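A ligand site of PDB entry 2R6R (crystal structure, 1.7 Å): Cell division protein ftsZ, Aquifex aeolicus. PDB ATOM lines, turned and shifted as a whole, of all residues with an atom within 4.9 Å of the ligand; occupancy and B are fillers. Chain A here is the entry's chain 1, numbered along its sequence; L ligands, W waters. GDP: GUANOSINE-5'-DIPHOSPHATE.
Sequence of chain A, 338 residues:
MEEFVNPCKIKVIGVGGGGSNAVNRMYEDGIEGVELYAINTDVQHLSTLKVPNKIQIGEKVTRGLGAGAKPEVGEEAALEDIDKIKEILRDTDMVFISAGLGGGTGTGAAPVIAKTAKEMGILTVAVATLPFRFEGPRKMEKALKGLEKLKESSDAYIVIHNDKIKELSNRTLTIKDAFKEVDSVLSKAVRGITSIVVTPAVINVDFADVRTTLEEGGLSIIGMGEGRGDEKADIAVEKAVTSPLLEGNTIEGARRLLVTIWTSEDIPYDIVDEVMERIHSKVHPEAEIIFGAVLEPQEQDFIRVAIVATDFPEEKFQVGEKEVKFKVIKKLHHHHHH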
ATOM      1  N   VAL A  15      -4.508  19.518   1.568  1.00  0.00           N
ATOM      2  CA  VAL A  15      -3.092  19.774   1.339  1.00  0.00           C
ATOM      3  C   VAL A  15      -2.774  19.714  -0.170  1.00  0.00           C
ATOM      4  O   VAL A  15      -2.947  18.656  -0.791  1.00  0.00           O
ATOM      5  CB  VAL A  15      -2.208  18.756   2.088  1.00  0.00           C
ATOM      6  CG1 VAL A  15      -0.710  19.104   1.924  1.00  0.00           C
ATOM      7  CG2 VAL A  15      -2.604  18.694   3.552  1.00  0.00           C
ATOM      8  N   GLY A  16      -2.300  20.835  -0.745  1.00  0.00           N
ATOM      9  CA  GLY A  16      -2.075  20.911  -2.185  1.00  0.00           C
ATOM     10  C   GLY A  16      -3.358  21.229  -2.943  1.00  0.00           C
ATOM     11  O   GLY A  16      -4.410  21.453  -2.328  1.00  0.00           O
ATOM     12  N   GLY A  17      -3.274  21.239  -4.273  1.00  0.00           N
ATOM     13  CA  GLY A  17      -4.398  21.718  -5.093  1.00  0.00           C
ATOM     14  C   GLY A  17      -5.587  20.785  -5.013  1.00  0.00           C
ATOM     15  O   GLY A  17      -6.718  21.220  -4.805  1.00  0.00           O
ATOM     16  N   GLY A  18      -5.322  19.487  -5.191  1.00  0.00           N
ATOM     17  CA  GLY A  18      -6.404  18.503  -5.173  1.00  0.00           C
ATOM     18  C   GLY A  18      -7.087  18.462  -3.823  1.00  0.00           C
ATOM     19  O   GLY A  18      -8.304  18.518  -3.741  1.00  0.00           O
ATOM     20  N   GLY A  19      -6.285  18.378  -2.753  1.00  0.00           N
ATOM     21  CA  GLY A  19      -6.803  18.329  -1.368  1.00  0.00           C
ATOM     22  C   GLY A  19      -7.625  19.580  -1.048  1.00  0.00           C
ATOM     23  O   GLY A  19      -8.702  19.518  -0.446  1.00  0.00           O
ATOM     24  N   ASN A  21      -9.078  21.538  -3.251  1.00  0.00           N
ATOM     25  CA  ASN A  21     -10.314  21.474  -4.021  1.00  0.00           C
ATOM     26  C   ASN A  21     -11.371  20.593  -3.361  1.00  0.00           C
ATOM     27  O   ASN A  21     -12.559  20.952  -3.345  1.00  0.00           O
ATOM     28  CB  ASN A  21     -10.051  21.115  -5.481  1.00  0.00           C
ATOM     29  CG  ASN A  21      -9.467  22.278  -6.254  1.00  0.00           C
ATOM     30  OD1 ASN A  21      -9.431  23.422  -5.766  1.00  0.00           O
ATOM     31  ND2 ASN A  21      -9.017  22.009  -7.481  1.00  0.00           N
ATOM     32  N   ALA A  22     -10.948  19.478  -2.760  1.00  0.00           N
ATOM     33  CA  ALA A  22     -11.885  18.578  -2.085  1.00  0.00           C
ATOM     34  C   ALA A  22     -12.488  19.252  -0.863  1.00  0.00           C
ATOM     35  O   ALA A  22     -13.711  19.171  -0.609  1.00  0.00           O
ATOM     36  CB  ALA A  22     -11.184  17.251  -1.694  1.00  0.00           C
ATOM     37  N   ASN A  40      -1.255  25.195   1.108  1.00  0.00           N
ATOM     38  CA  ASN A  40      -0.606  25.016  -0.196  1.00  0.00           C
ATOM     39  C   ASN A  40       0.689  25.801  -0.253  1.00  0.00           C
ATOM     40  O   ASN A  40       0.858  26.789   0.482  1.00  0.00           O
ATOM     41  CB  ASN A  40      -1.565  25.505  -1.297  1.00  0.00           C
ATOM     42  CG  ASN A  40      -1.388  24.784  -2.644  1.00  0.00           C
ATOM     43  OD1 ASN A  40      -2.337  24.730  -3.466  1.00  0.00           O
ATOM     44  ND2 ASN A  40      -0.206  24.251  -2.891  1.00  0.00           N
ATOM     45  N   ALA A  69       5.516  19.926  -8.615  1.00  0.00           N
ATOM     46  CA  ALA A  69       5.194  18.494  -8.567  1.00  0.00           C
ATOM     47  C   ALA A  69       6.275  17.628  -7.894  1.00  0.00           C
ATOM     48  O   ALA A  69       6.283  16.404  -8.053  1.00  0.00           O
ATOM     49  CB  ALA A  69       4.854  17.957  -9.971  1.00  0.00           C
ATOM     50  N   GLY A 100      -4.467  14.864  -2.689  1.00  0.00           N
ATOM     51  CA  GLY A 100      -4.392  14.140  -3.946  1.00  0.00           C
ATOM     52  C   GLY A 100      -2.946  13.707  -4.139  1.00  0.00           C
ATOM     53  O   GLY A 100      -2.076  14.544  -4.407  1.00  0.00           O
ATOM     54  N   LEU A 101      -2.670  12.420  -3.937  1.00  0.00           N
ATOM     55  CA  LEU A 101      -1.308  11.939  -4.051  1.00  0.00           C
ATOM     56  C   LEU A 101      -0.878  11.886  -5.508  1.00  0.00           C
ATOM     57  O   LEU A 101      -1.688  11.635  -6.407  1.00  0.00           O
ATOM     58  CB  LEU A 101      -1.100  10.583  -3.371  1.00  0.00           C
ATOM     59  CG  LEU A 101      -1.501  10.550  -1.891  1.00  0.00           C
ATOM     60  CD1 LEU A 101      -1.180   9.158  -1.304  1.00  0.00           C
ATOM     61  CD2 LEU A 101      -0.793  11.643  -1.136  1.00  0.00           C
ATOM     62  N   GLY A 102       0.404  12.177  -5.720  1.00  0.00           N
ATOM     63  CA  GLY A 102       0.945  12.180  -7.088  1.00  0.00           C
ATOM     64  C   GLY A 102       1.488  13.521  -7.551  1.00  0.00           C
ATOM     65  O   GLY A 102       2.151  13.589  -8.588  1.00  0.00           O
ATOM     66  N   GLY A 103       1.216  14.584  -6.786  1.00  0.00           N
ATOM     67  CA  GLY A 103       1.767  15.914  -7.049  1.00  0.00           C
ATOM     68  C   GLY A 103       2.937  16.157  -6.106  1.00  0.00           C
ATOM     69  O   GLY A 103       3.523  15.216  -5.575  1.00  0.00           O
ATOM     70  N   GLY A 104       3.236  17.430  -5.865  1.00  0.00           N
ATOM     71  CA  GLY A 104       4.352  17.754  -4.976  1.00  0.00           C
ATOM     72  C   GLY A 104       3.953  18.089  -3.564  1.00  0.00           C
ATOM     73  O   GLY A 104       4.526  17.585  -2.603  1.00  0.00           O
ATOM     74  N   THR A 105       2.993  19.002  -3.432  1.00  0.00           N
ATOM     75  CA  THR A 105       2.626  19.539  -2.146  1.00  0.00           C
ATOM     76  C   THR A 105       1.870  18.513  -1.318  1.00  0.00           C
ATOM     77  O   THR A 105       2.218  18.278  -0.148  1.00  0.00           O
ATOM     78  CB  THR A 105       1.794  20.840  -2.348  1.00  0.00           C
ATOM     79  OG1 THR A 105       2.598  21.780  -3.078  1.00  0.00           O
ATOM     80  CG2 THR A 105       1.384  21.426  -1.018  1.00  0.00           C
ATOM     81  N   GLY A 106       0.819  17.927  -1.884  1.00  0.00           N
ATOM     82  CA  GLY A 106       0.063  16.887  -1.171  1.00  0.00           C
ATOM     83  C   GLY A 106       0.973  15.723  -0.809  1.00  0.00           C
ATOM     84  O   GLY A 106       1.128  15.361   0.373  1.00  0.00           O
ATOM     85  N   THR A 107       1.649  15.178  -1.791  1.00  0.00           N
ATOM     86  CA  THR A 107       2.497  13.987  -1.612  1.00  0.00           C
ATOM     87  C   THR A 107       3.567  14.247  -0.537  1.00  0.00           C
ATOM     88  O   THR A 107       3.761  13.414   0.360  1.00  0.00           O
ATOM     89  CB  THR A 107       3.186  13.560  -2.926  1.00  0.00           C
ATOM     90  OG1 THR A 107       2.216  13.504  -3.996  1.00  0.00           O
ATOM     91  CG2 THR A 107       3.851  12.174  -2.745  1.00  0.00           C
ATOM     92  N   THR A 129      -6.142  10.320  -2.319  1.00  0.00           N
ATOM     93  CA  THR A 129      -6.470   9.737  -3.603  1.00  0.00           C
ATOM     94  C   THR A 129      -5.217   9.296  -4.358  1.00  0.00           C
ATOM     95  O   THR A 129      -4.155   9.900  -4.210  1.00  0.00           O
ATOM     96  CB  THR A 129      -7.305  10.655  -4.528  1.00  0.00           C
ATOM     97  OG1 THR A 129      -6.547  11.821  -4.902  1.00  0.00           O
ATOM     98  CG2 THR A 129      -8.642  11.038  -3.882  1.00  0.00           C
ATOM     99  N   PRO A 131      -4.026   8.718  -8.443  1.00  0.00           N
ATOM    100  CA  PRO A 131      -4.454   9.341  -9.695  1.00  0.00           C
ATOM    101  C   PRO A 131      -5.177   8.435 -10.697  1.00  0.00           C
ATOM    102  O   PRO A 131      -5.038   7.193 -10.650  1.00  0.00           O
ATOM    103  CB  PRO A 131      -3.129   9.857 -10.315  1.00  0.00           C
ATOM    104  CG  PRO A 131      -2.060   8.949  -9.698  1.00  0.00           C
ATOM    105  CD  PRO A 131      -2.558   8.737  -8.289  1.00  0.00           C
ATOM    106  N   PHE A 132      -5.946   9.077 -11.572  1.00  0.00           N
ATOM    107  CA  PHE A 132      -6.546   8.443 -12.743  1.00  0.00           C
ATOM    108  C   PHE A 132      -5.484   7.835 -13.666  1.00  0.00           C
ATOM    109  O   PHE A 132      -4.345   8.319 -13.743  1.00  0.00           O
ATOM    110  CB  PHE A 132      -7.315   9.477 -13.570  1.00  0.00           C
ATOM    111  CG  PHE A 132      -8.580   9.995 -12.928  1.00  0.00           C
ATOM    112  CD1 PHE A 132      -9.753   9.238 -12.942  1.00  0.00           C
ATOM    113  CD2 PHE A 132      -8.631  11.300 -12.422  1.00  0.00           C
ATOM    114  CE1 PHE A 132     -10.939   9.752 -12.408  1.00  0.00           C
ATOM    115  CE2 PHE A 132      -9.801  11.809 -11.891  1.00  0.00           C
ATOM    116  CZ  PHE A 132     -10.973  11.040 -11.869  1.00  0.00           C
ATOM    117  N   GLU A 135      -3.582  10.192 -15.991  1.00  0.00           N
ATOM    118  CA  GLU A 135      -2.548  11.053 -15.419  1.00  0.00           C
ATOM    119  C   GLU A 135      -1.151  10.468 -15.547  1.00  0.00           C
ATOM    120  O   GLU A 135      -0.166  11.125 -15.242  1.00  0.00           O
ATOM    121  CB  GLU A 135      -2.862  11.335 -13.952  1.00  0.00           C
ATOM    122  CG  GLU A 135      -4.135  12.032 -13.737  1.00  0.00           C
ATOM    123  CD  GLU A 135      -4.261  12.523 -12.301  1.00  0.00           C
ATOM    124  OE1 GLU A 135      -3.526  13.471 -11.933  1.00  0.00           O
ATOM    125  OE2 GLU A 135      -5.127  11.991 -11.563  1.00  0.00           O
ATOM    126  N   LYS A 139       3.020   9.835 -12.107  1.00  0.00           N
ATOM    127  CA  LYS A 139       2.188  10.340 -11.018  1.00  0.00           C
ATOM    128  C   LYS A 139       1.765   9.192 -10.108  1.00  0.00           C
ATOM    129  O   LYS A 139       1.780   9.341  -8.894  1.00  0.00           O
ATOM    130  CB  LYS A 139       0.992  11.133 -11.527  1.00  0.00           C
ATOM    131  CG  LYS A 139       1.400  12.414 -12.304  1.00  0.00           C
ATOM    132  CD  LYS A 139       0.230  13.369 -12.449  1.00  0.00           C
ATOM    133  CE  LYS A 139       0.063  14.215 -11.224  1.00  0.00           C
ATOM    134  NZ  LYS A 139       1.160  15.202 -11.057  1.00  0.00           N
ATOM    135  N   ASN A 162      -8.826   6.978  -7.983  1.00  0.00           N
ATOM    136  CA  ASN A 162      -9.720   7.773  -8.856  1.00  0.00           C
ATOM    137  C   ASN A 162     -10.369   6.989  -9.999  1.00  0.00           C
ATOM    138  O   ASN A 162     -11.526   7.277 -10.384  1.00  0.00           O
ATOM    139  CB  ASN A 162      -8.976   8.998  -9.420  1.00  0.00           C
ATOM    140  CG  ASN A 162      -8.683  10.042  -8.354  1.00  0.00           C
ATOM    141  OD1 ASN A 162      -9.174   9.953  -7.219  1.00  0.00           O
ATOM    142  ND2 ASN A 162      -7.915  11.065  -8.732  1.00  0.00           N
ATOM    143  N   PHE A 179     -12.797  15.516 -12.058  1.00  0.00           N
ATOM    144  CA  PHE A 179     -12.361  15.833 -10.681  1.00  0.00           C
ATOM    145  C   PHE A 179     -13.501  16.297  -9.796  1.00  0.00           C
ATOM    146  O   PHE A 179     -13.450  16.143  -8.571  1.00  0.00           O
ATOM    147  CB  PHE A 179     -11.165  16.794 -10.676  1.00  0.00           C
ATOM    148  CG  PHE A 179      -9.869  16.135 -11.074  1.00  0.00           C
ATOM    149  CD1 PHE A 179      -9.293  15.182 -10.233  1.00  0.00           C
ATOM    150  CD2 PHE A 179      -9.232  16.455 -12.277  1.00  0.00           C
ATOM    151  CE1 PHE A 179      -8.086  14.558 -10.572  1.00  0.00           C
ATOM    152  CE2 PHE A 179      -8.025  15.852 -12.622  1.00  0.00           C
ATOM    153  CZ  PHE A 179      -7.444  14.880 -11.782  1.00  0.00           C
ATOM    154  N   VAL A 182     -14.750  13.228  -8.178  1.00  0.00           N
ATOM    155  CA  VAL A 182     -13.803  12.903  -7.095  1.00  0.00           C
ATOM    156  C   VAL A 182     -14.104  13.774  -5.867  1.00  0.00           C
ATOM    157  O   VAL A 182     -14.276  13.233  -4.750  1.00  0.00           O
ATOM    158  CB  VAL A 182     -12.309  13.017  -7.526  1.00  0.00           C
ATOM    159  CG1 VAL A 182     -11.417  12.617  -6.326  1.00  0.00           C
ATOM    160  CG2 VAL A 182     -12.004  12.049  -8.677  1.00  0.00           C
ATOM    161  N   ASP A 183     -14.193  15.100  -6.044  1.00  0.00           N
ATOM    162  CA  ASP A 183     -14.489  16.030  -4.909  1.00  0.00           C
ATOM    163  C   ASP A 183     -15.775  15.595  -4.232  1.00  0.00           C
ATOM    164  O   ASP A 183     -15.873  15.567  -3.014  1.00  0.00           O
ATOM    165  CB  ASP A 183     -14.705  17.464  -5.379  1.00  0.00           C
ATOM    166  CG  ASP A 183     -13.473  18.090  -6.009  1.00  0.00           C
ATOM    167  OD1 ASP A 183     -12.328  17.593  -5.818  1.00  0.00           O
ATOM    168  OD2 ASP A 183     -13.657  19.111  -6.718  1.00  0.00           O
ATOM    169  N   LEU A 186     -15.211  12.378  -2.085  1.00  0.00           N
ATOM    170  CA  LEU A 186     -14.396  12.707  -0.906  1.00  0.00           C
ATOM    171  C   LEU A 186     -15.221  13.467   0.128  1.00  0.00           C
ATOM    172  O   LEU A 186     -15.158  13.203   1.334  1.00  0.00           O
ATOM    173  CB  LEU A 186     -13.201  13.538  -1.326  1.00  0.00           C
ATOM    174  CG  LEU A 186     -12.206  12.774  -2.210  1.00  0.00           C
ATOM    175  CD1 LEU A 186     -11.147  13.742  -2.762  1.00  0.00           C
ATOM    176  CD2 LEU A 186     -11.549  11.632  -1.471  1.00  0.00           C
HETATM  177  PB  GDP L   1      -0.013  19.354  -5.533  1.00  0.00           P
HETATM  178  O1B GDP L   1       1.464  19.498  -5.846  1.00  0.00           O
HETATM  179  O2B GDP L   1      -0.658  20.699  -5.452  1.00  0.00           O
HETATM  180  O3B GDP L   1      -0.238  18.503  -4.332  1.00  0.00           O
HETATM  181  O3A GDP L   1      -0.666  18.596  -6.783  1.00  0.00           O
HETATM  182  PA  GDP L   1      -2.256  18.476  -7.031  1.00  0.00           P
HETATM  183  O1A GDP L   1      -3.013  18.377  -5.732  1.00  0.00           O
HETATM  184  O2A GDP L   1      -2.721  19.589  -7.955  1.00  0.00           O
HETATM  185  O5' GDP L   1      -2.339  17.133  -7.857  1.00  0.00           O
HETATM  186  C5' GDP L   1      -2.112  15.889  -7.223  1.00  0.00           C
HETATM  187  C4' GDP L   1      -3.235  14.913  -7.514  1.00  0.00           C
HETATM  188  O4' GDP L   1      -4.465  15.450  -7.029  1.00  0.00           O
HETATM  189  C3' GDP L   1      -3.438  14.752  -9.017  1.00  0.00           C
HETATM  190  O3' GDP L   1      -2.548  13.770  -9.533  1.00  0.00           O
HETATM  191  C2' GDP L   1      -4.913  14.397  -9.159  1.00  0.00           C
HETATM  192  O2' GDP L   1      -5.162  12.978  -9.145  1.00  0.00           O
HETATM  193  C1' GDP L   1      -5.511  15.083  -7.930  1.00  0.00           C
HETATM  194  N9  GDP L   1      -6.285  16.295  -8.288  1.00  0.00           N
HETATM  195  C8  GDP L   1      -5.957  17.278  -9.154  1.00  0.00           C
HETATM  196  N7  GDP L   1      -6.934  18.228  -9.184  1.00  0.00           N
HETATM  197  C5  GDP L   1      -7.903  17.807  -8.340  1.00  0.00           C
HETATM  198  C6  GDP L   1      -9.208  18.327  -7.920  1.00  0.00           C
HETATM  199  O6  GDP L   1      -9.647  19.388  -8.397  1.00  0.00           O
HETATM  200  N1  GDP L   1      -9.899  17.615  -7.021  1.00  0.00           N
HETATM  201  C2  GDP L   1      -9.450  16.440  -6.505  1.00  0.00           C
HETATM  202  N2  GDP L   1     -10.210  15.761  -5.608  1.00  0.00           N
HETATM  203  N3  GDP L   1      -8.259  15.894  -6.847  1.00  0.00           N
HETATM  204  C4  GDP L   1      -7.461  16.542  -7.751  1.00  0.00           C
HETATM  205  O   HOH W   1       0.253  15.807  -4.257  1.00  0.00           O
HETATM  206  O   HOH W   2      -7.931  14.123  -4.591  1.00  0.00           O
HETATM  207  O   HOH W   3     -12.224  20.185  -8.701  1.00  0.00           O
HETATM  208  O   HOH W   4       1.888  18.873  -8.688  1.00  0.00           O
HETATM  209  O   HOH W   5      -4.610  11.510  -6.776  1.00  0.00           O
HETATM  210  O   HOH W   6       3.556  21.072  -6.921  1.00  0.00           O
HETATM  211  O   HOH W   7      -3.554  17.533  -3.181  1.00  0.00           O
HETATM  212  O   HOH W   8       0.896  22.825  -4.873  1.00  0.00           O
HETATM  213  O   HOH W   9      -1.351  21.843  -7.750  1.00  0.00           O
HETATM  214  O   HOH W  10      -5.197  20.889  -8.904  1.00  0.00           O
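The backbone NH (N) of Leu 101 lies within hydrogen-bond range of the backbone carbonyl oxygen (O) of Thr 129 (2.9 Å). The backbone carbonyl oxygen (O) of Gly 103 is in hydrogen-bond range of the side-chain hydroxyl (OG1) of Thr 107. The side-chain carboxylate (OE2) of Glu 135 sits at hydrogen-bond distance from the backbone NH (N) of Phe 132 (3.0 Å). O of Gly 102 sits at hydrogen-bond distance from NZ of Lys 139.
Water W8 lies within hydrogen-bond range of ND2 of Asn 40, OG1 of Thr 105 and O2B of the ligand. Water W3 bridges the side-chain carboxylate (OD2) of Asp 183 (2.7 Å) and an oxygen (O6) of the ligand (2.7 Å). Water W6 lies within hydrogen-bond range of O1B of the ligand and N of Ala 69. Water W5 lies within hydrogen-bond range of the side-chain hydroxyl of Thr 129 (2.7 Å), an oxygen (O2') of the ligand (2.8 Å) and the backbone carbonyl oxygen of Leu 101 (2.9 Å). Water W2 lies within hydrogen-bond range of OG1 of Thr 129 (2.7 Å) and N3 of the ligand (2.9 Å). Water W4 bridges O1B of the ligand (2.9 Å) and N of Gly 104 (3.4 Å).
O1A of the ligand sits at hydrogen-bond distance from N of Gly 18, 2.6 Å away. The side-chain carboxylate (OD1) of Asp 183 sits at hydrogen-bond distance from a nitrogen (N1) of the ligand. OE1 of Glu 135 is in hydrogen-bond range of O3' of the ligand, at 2.6 Å. The backbone NH (N) of Gly 106 sits at hydrogen-bond distance from an oxygen (O3B) of the ligand. O1B of the ligand lies within hydrogen-bond range of N of Gly 104 (2.7 Å). O1B of the ligand sits at hydrogen-bond distance from N of Thr 105, 2.9 Å away. The backbone NH (N) of Gly 17 is in hydrogen-bond range of an oxygen (O2B) of the ligand (2.9 Å). ND2 of Asn 162 is in hydrogen-bond range of O2' of the ligand, at 3.4 Å. An oxygen (O6) of the ligand sits at hydrogen-bond distance from the side-chain amide nitrogen (ND2) of Asn 21 (2.8 Å).
CA of Gly 16 touches O2B of the ligand (3.6 Å). Gly 100 touches the ligand. Leu 101 touches the ligand. Gly 103 touches the ligand (N to C5', 3.6 Å). Pro 131 touches the ligand (CA to O2', 3.7 Å). CE of Lys 139 touches O3' of the ligand (3.1 Å). CD1 of Phe 179 touches C4 of the ligand, 3.4 Å away. Val 182 touches the ligand. Leu 186 touches the ligand. Hydrophobic or aromatic side chains that line the ligand: Pro 131, Phe 179, Val 182 and Leu 186. Of the 27 residues printed, 18 come within 4 Å of the ligand. The nearest printed residue that does not touch the ligand is Ala 22 (4.3 Å).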
